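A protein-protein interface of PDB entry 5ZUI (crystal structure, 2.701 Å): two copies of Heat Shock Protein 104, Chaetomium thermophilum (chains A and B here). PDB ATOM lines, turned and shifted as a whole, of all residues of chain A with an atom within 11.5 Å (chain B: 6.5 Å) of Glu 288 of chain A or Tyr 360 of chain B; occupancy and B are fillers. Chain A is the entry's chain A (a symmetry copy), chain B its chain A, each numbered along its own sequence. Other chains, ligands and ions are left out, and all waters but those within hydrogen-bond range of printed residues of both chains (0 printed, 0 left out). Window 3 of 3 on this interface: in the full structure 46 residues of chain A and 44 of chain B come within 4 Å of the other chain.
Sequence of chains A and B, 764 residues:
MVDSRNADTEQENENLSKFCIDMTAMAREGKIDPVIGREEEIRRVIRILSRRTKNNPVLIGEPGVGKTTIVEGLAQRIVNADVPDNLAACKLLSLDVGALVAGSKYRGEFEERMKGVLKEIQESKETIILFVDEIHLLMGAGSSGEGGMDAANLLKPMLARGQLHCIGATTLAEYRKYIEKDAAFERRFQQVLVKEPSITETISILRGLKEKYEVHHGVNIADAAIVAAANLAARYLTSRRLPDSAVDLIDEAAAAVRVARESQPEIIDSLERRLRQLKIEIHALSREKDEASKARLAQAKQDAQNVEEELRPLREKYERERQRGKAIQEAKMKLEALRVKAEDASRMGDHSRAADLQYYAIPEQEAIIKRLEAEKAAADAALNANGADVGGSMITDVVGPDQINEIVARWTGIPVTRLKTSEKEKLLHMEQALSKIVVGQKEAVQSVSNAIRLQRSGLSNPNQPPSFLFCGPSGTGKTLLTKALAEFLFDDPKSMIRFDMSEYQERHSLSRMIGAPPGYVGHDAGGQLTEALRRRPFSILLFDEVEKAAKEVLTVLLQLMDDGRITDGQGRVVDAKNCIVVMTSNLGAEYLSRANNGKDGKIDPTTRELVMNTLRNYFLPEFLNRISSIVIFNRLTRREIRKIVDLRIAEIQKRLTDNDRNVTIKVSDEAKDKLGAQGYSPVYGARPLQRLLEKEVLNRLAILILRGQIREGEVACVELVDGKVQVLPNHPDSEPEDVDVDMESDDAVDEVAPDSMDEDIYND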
ATOM      1  N   LEU A 278     -19.276  -6.711 -32.273  1.00  0.00           N
ATOM      2  CA  LEU A 278     -20.734  -6.745 -32.198  1.00  0.00           C
ATOM      3  C   LEU A 278     -21.215  -7.000 -30.776  1.00  0.00           C
ATOM      4  O   LEU A 278     -22.248  -6.458 -30.366  1.00  0.00           O
ATOM      5  CB  LEU A 278     -21.285  -7.801 -33.153  1.00  0.00           C
ATOM      6  CG  LEU A 278     -21.016  -7.526 -34.632  1.00  0.00           C
ATOM      7  CD1 LEU A 278     -21.106  -8.812 -35.453  1.00  0.00           C
ATOM      8  CD2 LEU A 278     -21.970  -6.479 -35.155  1.00  0.00           C
ATOM      9  N   LYS A 279     -20.480  -7.793 -29.999  1.00  0.00           N
ATOM     10  CA  LYS A 279     -20.862  -7.980 -28.605  1.00  0.00           C
ATOM     11  C   LYS A 279     -20.770  -6.670 -27.826  1.00  0.00           C
ATOM     12  O   LYS A 279     -21.585  -6.418 -26.931  1.00  0.00           O
ATOM     13  CB  LYS A 279     -19.996  -9.063 -27.958  1.00  0.00           C
ATOM     14  CG  LYS A 279     -20.227 -10.466 -28.509  1.00  0.00           C
ATOM     15  CD  LYS A 279     -19.705 -11.522 -27.552  1.00  0.00           C
ATOM     16  CE  LYS A 279     -19.696 -12.908 -28.179  1.00  0.00           C
ATOM     17  NZ  LYS A 279     -19.003 -13.880 -27.289  1.00  0.00           N
ATOM     18  N   ILE A 280     -19.789  -5.820 -28.150  1.00  0.00           N
ATOM     19  CA  ILE A 280     -19.720  -4.492 -27.537  1.00  0.00           C
ATOM     20  C   ILE A 280     -20.924  -3.654 -27.953  1.00  0.00           C
ATOM     21  O   ILE A 280     -21.597  -3.036 -27.118  1.00  0.00           O
ATOM     22  CB  ILE A 280     -18.406  -3.780 -27.909  1.00  0.00           C
ATOM     23  CG1 ILE A 280     -17.187  -4.632 -27.560  1.00  0.00           C
ATOM     24  CG2 ILE A 280     -18.336  -2.414 -27.216  1.00  0.00           C
ATOM     25  CD1 ILE A 280     -17.105  -4.987 -26.119  1.00  0.00           C
ATOM     26  N   GLU A 281     -21.199  -3.604 -29.262  1.00  0.00           N
ATOM     27  CA  GLU A 281     -22.323  -2.823 -29.762  1.00  0.00           C
ATOM     28  C   GLU A 281     -23.652  -3.314 -29.197  1.00  0.00           C
ATOM     29  O   GLU A 281     -24.555  -2.506 -28.951  1.00  0.00           O
ATOM     30  CB  GLU A 281     -22.340  -2.862 -31.291  1.00  0.00           C
ATOM     31  CG  GLU A 281     -23.470  -2.052 -31.911  1.00  0.00           C
ATOM     32  CD  GLU A 281     -23.390  -1.980 -33.425  1.00  0.00           C
ATOM     33  OE1 GLU A 281     -22.624  -2.760 -34.028  1.00  0.00           O
ATOM     34  OE2 GLU A 281     -24.100  -1.137 -34.013  1.00  0.00           O
ATOM     35  N   ILE A 282     -23.789  -4.624 -28.976  1.00  0.00           N
ATOM     36  CA  ILE A 282     -25.032  -5.168 -28.437  1.00  0.00           C
ATOM     37  C   ILE A 282     -25.256  -4.674 -27.013  1.00  0.00           C
ATOM     38  O   ILE A 282     -26.351  -4.221 -26.662  1.00  0.00           O
ATOM     39  CB  ILE A 282     -25.014  -6.708 -28.513  1.00  0.00           C
ATOM     40  CG1 ILE A 282     -25.366  -7.170 -29.928  1.00  0.00           C
ATOM     41  CG2 ILE A 282     -25.950  -7.324 -27.473  1.00  0.00           C
ATOM     42  CD1 ILE A 282     -24.752  -8.503 -30.304  1.00  0.00           C
ATOM     43  N   HIS A 283     -24.220  -4.752 -26.172  1.00  0.00           N
ATOM     44  CA  HIS A 283     -24.329  -4.245 -24.807  1.00  0.00           C
ATOM     45  C   HIS A 283     -24.674  -2.761 -24.779  1.00  0.00           C
ATOM     46  O   HIS A 283     -25.377  -2.302 -23.872  1.00  0.00           O
ATOM     47  CB  HIS A 283     -23.022  -4.479 -24.058  1.00  0.00           C
ATOM     48  CG  HIS A 283     -23.030  -5.690 -23.186  1.00  0.00           C
ATOM     49  ND1 HIS A 283     -22.577  -6.918 -23.616  1.00  0.00           N
ATOM     50  CD2 HIS A 283     -23.410  -5.859 -21.897  1.00  0.00           C
ATOM     51  CE1 HIS A 283     -22.686  -7.793 -22.634  1.00  0.00           C
ATOM     52  NE2 HIS A 283     -23.190  -7.178 -21.580  1.00  0.00           N
ATOM     53  N   ALA A 284     -24.180  -1.997 -25.755  1.00  0.00           N
ATOM     54  CA  ALA A 284     -24.422  -0.561 -25.772  1.00  0.00           C
ATOM     55  C   ALA A 284     -25.813  -0.233 -26.297  1.00  0.00           C
ATOM     56  O   ALA A 284     -26.511   0.608 -25.722  1.00  0.00           O
ATOM     57  CB  ALA A 284     -23.359   0.141 -26.617  1.00  0.00           C
ATOM     58  N   LEU A 285     -26.220  -0.883 -27.391  1.00  0.00           N
ATOM     59  CA  LEU A 285     -27.531  -0.624 -27.973  1.00  0.00           C
ATOM     60  C   LEU A 285     -28.658  -0.994 -27.017  1.00  0.00           C
ATOM     61  O   LEU A 285     -29.701  -0.334 -27.007  1.00  0.00           O
ATOM     62  CB  LEU A 285     -27.673  -1.391 -29.286  1.00  0.00           C
ATOM     63  CG  LEU A 285     -27.125  -0.703 -30.535  1.00  0.00           C
ATOM     64  CD1 LEU A 285     -27.083  -1.670 -31.706  1.00  0.00           C
ATOM     65  CD2 LEU A 285     -27.962   0.516 -30.888  1.00  0.00           C
ATOM     66  N   SER A 286     -28.465  -2.031 -26.198  1.00  0.00           N
ATOM     67  CA  SER A 286     -29.499  -2.469 -25.265  1.00  0.00           C
ATOM     68  C   SER A 286     -29.803  -1.443 -24.182  1.00  0.00           C
ATOM     69  O   SER A 286     -30.700  -1.685 -23.366  1.00  0.00           O
ATOM     70  CB  SER A 286     -29.096  -3.788 -24.607  1.00  0.00           C
ATOM     71  OG  SER A 286     -28.211  -3.556 -23.523  1.00  0.00           O
ATOM     72  N   ARG A 287     -29.087  -0.322 -24.148  1.00  0.00           N
ATOM     73  CA  ARG A 287     -29.313   0.744 -23.179  1.00  0.00           C
ATOM     74  C   ARG A 287     -30.145   1.885 -23.738  1.00  0.00           C
ATOM     75  O   ARG A 287     -30.972   2.451 -23.018  1.00  0.00           O
ATOM     76  CB  ARG A 287     -27.976   1.303 -22.685  1.00  0.00           C
ATOM     77  CG  ARG A 287     -26.917   0.247 -22.454  1.00  0.00           C
ATOM     78  CD  ARG A 287     -25.788   0.800 -21.617  1.00  0.00           C
ATOM     79  NE  ARG A 287     -24.857  -0.243 -21.207  1.00  0.00           N
ATOM     80  CZ  ARG A 287     -23.578  -0.025 -20.933  1.00  0.00           C
ATOM     81  NH1 ARG A 287     -23.076   1.200 -21.027  1.00  0.00           N
ATOM     82  NH2 ARG A 287     -22.792  -1.029 -20.565  1.00  0.00           N
ATOM     83  N   GLU A 288     -29.947   2.235 -25.004  1.00  0.00           N
ATOM     84  CA  GLU A 288     -30.645   3.362 -25.600  1.00  0.00           C
ATOM     85  C   GLU A 288     -32.097   3.001 -25.897  1.00  0.00           C
ATOM     86  O   GLU A 288     -32.375   2.011 -26.578  1.00  0.00           O
ATOM     87  CB  GLU A 288     -29.929   3.809 -26.872  1.00  0.00           C
ATOM     88  CG  GLU A 288     -28.792   4.788 -26.611  1.00  0.00           C
ATOM     89  CD  GLU A 288     -27.662   4.648 -27.610  1.00  0.00           C
ATOM     90  OE1 GLU A 288     -27.953   4.416 -28.807  1.00  0.00           O
ATOM     91  OE2 GLU A 288     -26.484   4.766 -27.199  1.00  0.00           O
ATOM     92  N   LYS A 289     -33.018   3.813 -25.381  1.00  0.00           N
ATOM     93  CA  LYS A 289     -34.455   3.630 -25.583  1.00  0.00           C
ATOM     94  C   LYS A 289     -34.892   4.546 -26.723  1.00  0.00           C
ATOM     95  O   LYS A 289     -35.040   5.757 -26.539  1.00  0.00           O
ATOM     96  CB  LYS A 289     -35.217   3.928 -24.294  1.00  0.00           C
ATOM     97  CG  LYS A 289     -36.712   4.176 -24.473  1.00  0.00           C
ATOM     98  CD  LYS A 289     -37.495   2.876 -24.500  1.00  0.00           C
ATOM     99  CE  LYS A 289     -38.953   3.118 -24.847  1.00  0.00           C
ATOM    100  NZ  LYS A 289     -39.844   2.284 -23.997  1.00  0.00           N
ATOM    101  N   ASP A 290     -35.079   3.970 -27.905  1.00  0.00           N
ATOM    102  CA  ASP A 290     -35.622   4.693 -29.053  1.00  0.00           C
ATOM    103  C   ASP A 290     -35.997   3.667 -30.114  1.00  0.00           C
ATOM    104  O   ASP A 290     -35.740   2.472 -29.970  1.00  0.00           O
ATOM    105  CB  ASP A 290     -34.649   5.743 -29.604  1.00  0.00           C
ATOM    106  CG  ASP A 290     -33.273   5.182 -29.907  1.00  0.00           C
ATOM    107  OD1 ASP A 290     -32.545   4.841 -28.952  1.00  0.00           O
ATOM    108  OD2 ASP A 290     -32.913   5.098 -31.103  1.00  0.00           O
ATOM    109  N   GLU A 291     -36.602   4.153 -31.193  1.00  0.00           N
ATOM    110  CA  GLU A 291     -37.161   3.264 -32.205  1.00  0.00           C
ATOM    111  C   GLU A 291     -36.082   2.677 -33.109  1.00  0.00           C
ATOM    112  O   GLU A 291     -36.167   1.509 -33.502  1.00  0.00           O
ATOM    113  CB  GLU A 291     -38.205   4.025 -33.027  1.00  0.00           C
ATOM    114  CG  GLU A 291     -37.761   5.434 -33.463  1.00  0.00           C
ATOM    115  CD  GLU A 291     -38.041   6.520 -32.423  1.00  0.00           C
ATOM    116  OE1 GLU A 291     -38.569   6.204 -31.333  1.00  0.00           O
ATOM    117  OE2 GLU A 291     -37.725   7.697 -32.698  1.00  0.00           O
ATOM    118  N   ALA A 292     -35.064   3.472 -33.452  1.00  0.00           N
ATOM    119  CA  ALA A 292     -34.055   3.033 -34.410  1.00  0.00           C
ATOM    120  C   ALA A 292     -33.019   2.117 -33.779  1.00  0.00           C
ATOM    121  O   ALA A 292     -32.454   1.260 -34.468  1.00  0.00           O
ATOM    122  CB  ALA A 292     -33.357   4.246 -35.031  1.00  0.00           C
ATOM    123  N   SER A 293     -32.751   2.291 -32.484  1.00  0.00           N
ATOM    124  CA  SER A 293     -31.751   1.470 -31.811  1.00  0.00           C
ATOM    125  C   SER A 293     -32.226   0.031 -31.675  1.00  0.00           C
ATOM    126  O   SER A 293     -31.470  -0.916 -31.909  1.00  0.00           O
ATOM    127  CB  SER A 293     -31.439   2.061 -30.439  1.00  0.00           C
ATOM    128  OG  SER A 293     -30.600   3.195 -30.555  1.00  0.00           O
ATOM    129  N   LYS A 294     -33.479  -0.152 -31.296  1.00  0.00           N
ATOM    130  CA  LYS A 294     -34.004  -1.494 -31.105  1.00  0.00           C
ATOM    131  C   LYS A 294     -34.035  -2.268 -32.430  1.00  0.00           C
ATOM    132  O   LYS A 294     -33.736  -3.476 -32.455  1.00  0.00           O
ATOM    133  CB  LYS A 294     -35.367  -1.369 -30.452  1.00  0.00           C
ATOM    134  CG  LYS A 294     -35.332  -0.390 -29.241  1.00  0.00           C
ATOM    135  CD  LYS A 294     -34.704  -0.958 -28.005  1.00  0.00           C
ATOM    136  CE  LYS A 294     -33.246  -0.742 -27.783  1.00  0.00           C
ATOM    137  NZ  LYS A 294     -32.835  -1.310 -26.460  1.00  0.00           N
ATOM    138  N   ALA A 295     -34.314  -1.584 -33.554  1.00  0.00           N
ATOM    139  CA  ALA A 295     -34.396  -2.279 -34.836  1.00  0.00           C
ATOM    140  C   ALA A 295     -33.039  -2.754 -35.327  1.00  0.00           C
ATOM    141  O   ALA A 295     -32.994  -3.677 -36.143  1.00  0.00           O
ATOM    142  CB  ALA A 295     -35.039  -1.384 -35.880  1.00  0.00           C
ATOM    143  N   ARG A 296     -31.937  -2.138 -34.876  1.00  0.00           N
ATOM    144  CA  ARG A 296     -30.607  -2.604 -35.245  1.00  0.00           C
ATOM    145  C   ARG A 296     -29.941  -3.426 -34.148  1.00  0.00           C
ATOM    146  O   ARG A 296     -29.045  -4.224 -34.455  1.00  0.00           O
ATOM    147  CB  ARG A 296     -29.709  -1.418 -35.622  1.00  0.00           C
ATOM    148  CG  ARG A 296     -28.440  -1.808 -36.384  1.00  0.00           C
ATOM    149  CD  ARG A 296     -27.246  -1.942 -35.434  1.00  0.00           C
ATOM    150  NE  ARG A 296     -25.977  -2.172 -36.119  1.00  0.00           N
ATOM    151  CZ  ARG A 296     -25.547  -3.362 -36.534  1.00  0.00           C
ATOM    152  NH1 ARG A 296     -26.291  -4.447 -36.353  1.00  0.00           N
ATOM    153  NH2 ARG A 296     -24.369  -3.471 -37.136  1.00  0.00           N
ATOM    154  N   LEU A 297     -30.351  -3.254 -32.885  1.00  0.00           N
ATOM    155  CA  LEU A 297     -29.892  -4.165 -31.838  1.00  0.00           C
ATOM    156  C   LEU A 297     -30.278  -5.599 -32.159  1.00  0.00           C
ATOM    157  O   LEU A 297     -29.480  -6.524 -31.959  1.00  0.00           O
ATOM    158  CB  LEU A 297     -30.459  -3.755 -30.475  1.00  0.00           C
ATOM    159  CG  LEU A 297     -30.558  -4.845 -29.391  1.00  0.00           C
ATOM    160  CD1 LEU A 297     -29.192  -5.407 -29.030  1.00  0.00           C
ATOM    161  CD2 LEU A 297     -31.202  -4.285 -28.146  1.00  0.00           C
ATOM    162  N   ALA A 298     -31.498  -5.807 -32.651  1.00  0.00           N
ATOM    163  CA  ALA A 298     -31.887  -7.141 -33.081  1.00  0.00           C
ATOM    164  C   ALA A 298     -31.078  -7.575 -34.298  1.00  0.00           C
ATOM    165  O   ALA A 298     -30.712  -8.751 -34.426  1.00  0.00           O
ATOM    166  CB  ALA A 298     -33.386  -7.190 -33.375  1.00  0.00           C
ATOM    167  N   ALA A 300     -28.004  -6.581 -34.803  1.00  0.00           N
ATOM    168  CA  ALA A 300     -26.663  -6.847 -34.298  1.00  0.00           C
ATOM    169  C   ALA A 300     -26.556  -8.248 -33.707  1.00  0.00           C
ATOM    170  O   ALA A 300     -25.544  -8.935 -33.899  1.00  0.00           O
ATOM    171  CB  ALA A 300     -26.270  -5.792 -33.263  1.00  0.00           C
ATOM    172  N   ALA B 355     -18.365  -1.427 -23.354  1.00  0.00           N
ATOM    173  CA  ALA B 355     -19.399  -0.641 -24.013  1.00  0.00           C
ATOM    174  C   ALA B 355     -19.607   0.703 -23.330  1.00  0.00           C
ATOM    175  O   ALA B 355     -19.922   1.687 -24.007  1.00  0.00           O
ATOM    176  CB  ALA B 355     -20.714  -1.423 -24.057  1.00  0.00           C
ATOM    177  N   ASP B 356     -19.499   0.797 -22.017  1.00  0.00           N
ATOM    178  CA  ASP B 356     -19.519   2.067 -21.289  1.00  0.00           C
ATOM    179  C   ASP B 356     -18.547   3.066 -21.912  1.00  0.00           C
ATOM    180  O   ASP B 356     -18.930   4.172 -22.320  1.00  0.00           O
ATOM    181  CB  ASP B 356     -19.132   1.845 -19.818  1.00  0.00           C
ATOM    182  CG  ASP B 356     -20.216   1.155 -18.996  1.00  0.00           C
ATOM    183  OD1 ASP B 356     -21.133   0.555 -19.587  1.00  0.00           O
ATOM    184  OD2 ASP B 356     -20.130   1.187 -17.748  1.00  0.00           O
ATOM    185  N   LEU B 357     -17.272   2.669 -22.000  1.00  0.00           N
ATOM    186  CA  LEU B 357     -16.205   3.556 -22.431  1.00  0.00           C
ATOM    187  C   LEU B 357     -16.241   3.811 -23.938  1.00  0.00           C
ATOM    188  O   LEU B 357     -16.207   4.965 -24.372  1.00  0.00           O
ATOM    189  CB  LEU B 357     -14.865   2.966 -22.000  1.00  0.00           C
ATOM    190  CG  LEU B 357     -14.913   2.450 -20.555  1.00  0.00           C
ATOM    191  CD1 LEU B 357     -13.722   1.577 -20.208  1.00  0.00           C
ATOM    192  CD2 LEU B 357     -15.018   3.610 -19.572  1.00  0.00           C
ATOM    193  N   GLN B 358     -16.316   2.757 -24.756  1.00  0.00           N
ATOM    194  CA  GLN B 358     -16.165   2.939 -26.201  1.00  0.00           C
ATOM    195  C   GLN B 358     -17.313   3.714 -26.825  1.00  0.00           C
ATOM    196  O   GLN B 358     -17.141   4.288 -27.903  1.00  0.00           O
ATOM    197  CB  GLN B 358     -16.047   1.586 -26.907  1.00  0.00           C
ATOM    198  CG  GLN B 358     -14.699   0.888 -26.767  1.00  0.00           C
ATOM    199  CD  GLN B 358     -14.598  -0.357 -27.632  1.00  0.00           C
ATOM    200  OE1 GLN B 358     -15.284  -0.478 -28.652  1.00  0.00           O
ATOM    201  NE2 GLN B 358     -13.747  -1.295 -27.224  1.00  0.00           N
ATOM    202  N   TYR B 359     -18.478   3.738 -26.184  1.00  0.00           N
ATOM    203  CA  TYR B 359     -19.670   4.300 -26.799  1.00  0.00           C
ATOM    204  C   TYR B 359     -20.175   5.541 -26.087  1.00  0.00           C
ATOM    205  O   TYR B 359     -20.833   6.372 -26.722  1.00  0.00           O
ATOM    206  CB  TYR B 359     -20.797   3.250 -26.859  1.00  0.00           C
ATOM    207  CG  TYR B 359     -20.658   2.364 -28.082  1.00  0.00           C
ATOM    208  CD1 TYR B 359     -21.200   2.752 -29.302  1.00  0.00           C
ATOM    209  CD2 TYR B 359     -19.937   1.165 -28.030  1.00  0.00           C
ATOM    210  CE1 TYR B 359     -21.052   1.977 -30.440  1.00  0.00           C
ATOM    211  CE2 TYR B 359     -19.777   0.369 -29.173  1.00  0.00           C
ATOM    212  CZ  TYR B 359     -20.343   0.782 -30.377  1.00  0.00           C
ATOM    213  OH  TYR B 359     -20.203   0.016 -31.525  1.00  0.00           O
ATOM    214  N   TYR B 360     -19.857   5.700 -24.804  1.00  0.00           N
ATOM    215  CA  TYR B 360     -20.380   6.819 -24.036  1.00  0.00           C
ATOM    216  C   TYR B 360     -19.264   7.669 -23.420  1.00  0.00           C
ATOM    217  O   TYR B 360     -19.138   8.848 -23.759  1.00  0.00           O
ATOM    218  CB  TYR B 360     -21.356   6.290 -22.989  1.00  0.00           C
ATOM    219  CG  TYR B 360     -22.473   5.488 -23.622  1.00  0.00           C
ATOM    220  CD1 TYR B 360     -22.950   4.318 -23.041  1.00  0.00           C
ATOM    221  CD2 TYR B 360     -23.047   5.899 -24.817  1.00  0.00           C
ATOM    222  CE1 TYR B 360     -23.980   3.588 -23.645  1.00  0.00           C
ATOM    223  CE2 TYR B 360     -24.059   5.181 -25.428  1.00  0.00           C
ATOM    224  CZ  TYR B 360     -24.526   4.033 -24.842  1.00  0.00           C
ATOM    225  OH  TYR B 360     -25.537   3.358 -25.485  1.00  0.00           O
ATOM    226  N   ALA B 361     -18.441   7.099 -22.532  1.00  0.00           N
ATOM    227  CA  ALA B 361     -17.404   7.894 -21.868  1.00  0.00           C
ATOM    228  C   ALA B 361     -16.460   8.538 -22.876  1.00  0.00           C
ATOM    229  O   ALA B 361     -16.262   9.759 -22.866  1.00  0.00           O
ATOM    230  CB  ALA B 361     -16.611   7.030 -20.891  1.00  0.00           C
ATOM    231  N   ILE B 362     -15.863   7.726 -23.750  1.00  0.00           N
ATOM    232  CA  ILE B 362     -14.838   8.251 -24.652  1.00  0.00           C
ATOM    233  C   ILE B 362     -15.384   9.284 -25.625  1.00  0.00           C
ATOM    234  O   ILE B 362     -14.773  10.359 -25.753  1.00  0.00           O
ATOM    235  CB  ILE B 362     -14.108   7.071 -25.358  1.00  0.00           C
ATOM    236  CG1 ILE B 362     -13.154   6.397 -24.370  1.00  0.00           C
ATOM    237  CG2 ILE B 362     -13.361   7.529 -26.599  1.00  0.00           C
ATOM    238  CD1 ILE B 362     -12.584   5.092 -24.861  1.00  0.00           C
ATOM    239  N   PRO B 363     -16.506   9.065 -26.315  1.00  0.00           N
ATOM    240  CA  PRO B 363     -16.997  10.133 -27.206  1.00  0.00           C
ATOM    241  C   PRO B 363     -17.479  11.365 -26.456  1.00  0.00           C
ATOM    242  O   PRO B 363     -17.404  12.472 -27.006  1.00  0.00           O
ATOM    243  CB  PRO B 363     -18.136   9.455 -27.983  1.00  0.00           C
ATOM    244  CG  PRO B 363     -18.598   8.387 -27.086  1.00  0.00           C
ATOM    245  CD  PRO B 363     -17.369   7.872 -26.378  1.00  0.00           C
ATOM    246  N   GLU B 364     -17.974  11.210 -25.221  1.00  0.00           N
ATOM    247  CA  GLU B 364     -18.290  12.378 -24.406  1.00  0.00           C
ATOM    248  C   GLU B 364     -17.024  13.153 -24.069  1.00  0.00           C
ATOM    249  O   GLU B 364     -17.031  14.389 -24.038  1.00  0.00           O
ATOM    250  CB  GLU B 364     -19.039  11.956 -23.133  1.00  0.00           C
ATOM    251  CG  GLU B 364     -20.559  11.736 -23.343  1.00  0.00           C
ATOM    252  CD  GLU B 364     -21.216  10.860 -22.266  1.00  0.00           C
ATOM    253  OE1 GLU B 364     -20.586  10.618 -21.212  1.00  0.00           O
ATOM    254  OE2 GLU B 364     -22.364  10.402 -22.481  1.00  0.00           O
ATOM    255  N   GLN B 365     -15.954  12.430 -23.892  1.00  0.00           N
ATOM    256  CA  GLN B 365     -14.680  13.094 -23.660  1.00  0.00           C
ATOM    257  C   GLN B 365     -14.160  13.744 -24.936  1.00  0.00           C
ATOM    258  O   GLN B 365     -13.813  14.929 -24.934  1.00  0.00           O
ATOM    259  CB  GLN B 365     -13.672  12.093 -23.111  1.00  0.00           C
ATOM    260  CG  GLN B 365     -12.506  12.719 -22.395  1.00  0.00           C
ATOM    261  CD  GLN B 365     -12.919  13.615 -21.243  1.00  0.00           C
ATOM    262  OE1 GLN B 365     -12.320  14.663 -21.022  1.00  0.00           O
ATOM    263  NE2 GLN B 365     -13.935  13.203 -20.497  1.00  0.00           N
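The side-chain carboxylate (OD1) of Asp 356 of chain B lies within salt-bridge range of the guanidinium group (NH2) of Arg 287 of chain A (2.5 Å).
The side-chain hydroxyl of Tyr 360 of chain B sits at hydrogen-bond distance from the backbone carbonyl oxygen of Ala 284 of chain A (2.9 Å).
OH of Tyr 360 of chain B lies within hydrogen-bond range of OE2 of Glu 288 of chain A.
No position is printed for both chains.
Of the 11 pairs that touch across the chains among the printed residues, none has its exchanged pair printed and touching as well.
Glu 288 of chain A touches one residue of chain B.
Tyr 360 of chain B touches three residues of chain A.
Of the printed residues of chain A, Ala 355 of chain B touches Ile 280 (3.6 Å), His 283 (3.8 Å) and Ala 284 (3.9 Å).
Asp 356 of chain B touches just one residue of chain A: Arg 287 (2.5 Å).
No residue of chain A comes within 4 Å of Ile 362 of chain B.
No residue of chain A comes within 4 Å of Pro 363 of chain B.
Printed residues of chain B within 4 Å of His 283 of chain A: Ala 355.
Printed residues of chain A within 4 Å of Gln 358 of chain B: Ile 280 (3.9 Å).
Printed residues of chain A within 4 Å of Tyr 359 of chain B: Ile 280 (3.7 Å), Glu 281 (3.6 Å) and Ala 284 (3.8 Å).
Of the printed residues of chain B, Ile 280 of chain A touches Ala 355, Gln 358 and Tyr 359.
Gln 365 of chain B touches none of the printed residues of chain A.
Arg 296 of chain A touches none of the printed residues of chain B.
The nearest printed residue of chain A that does not touch Tyr 359 of chain B is Glu 288 of chain A (5.9 Å).
Among the printed residues, merely in contact across the chains: Ile 280 of chain A with Ala 355 of chain B, Glu 281 of chain A with Tyr 359 of chain B, Arg 287 of chain A with Tyr 360 of chain B, Ile 280 of chain A with Tyr 359 of chain B, Ala 284 of chain A with Tyr 359 of chain B, His 283 of chain A with Ala 355 of chain B, Ile 280 of chain A with Gln 358 of chain B and Ala 284 of chain A with Ala 355 of chain B.
Of the 22 printed residues of chain A, 6 touch a printed residue of chain B.
N of Ala 361 of chain B lies within hydrogen-bond range of O of Asp 356 of chain B (3.0 Å).
ND1 of His 283 of chain A is in hydrogen-bond range of O of Lys 279 of chain A (3.5 Å).
The side-chain carboxylate (OE2) of Glu 281 of chain A lies within salt-bridge range of the guanidinium group (NE) of Arg 296 of chain A.
The guanidinium group (NE) of Arg 287 of chain A sits close to the backbone carbonyl oxygen (O) of His 283 of chain A (3.4 Å).
The side-chain carboxylate of Glu 288 of chain A lies within hydrogen-bond range of the side-chain hydroxyl of Ser 293 of chain A (3.4 Å).
O of Glu 288 of chain A lies close to NZ of Lys 294 of chain A (3.4 Å).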
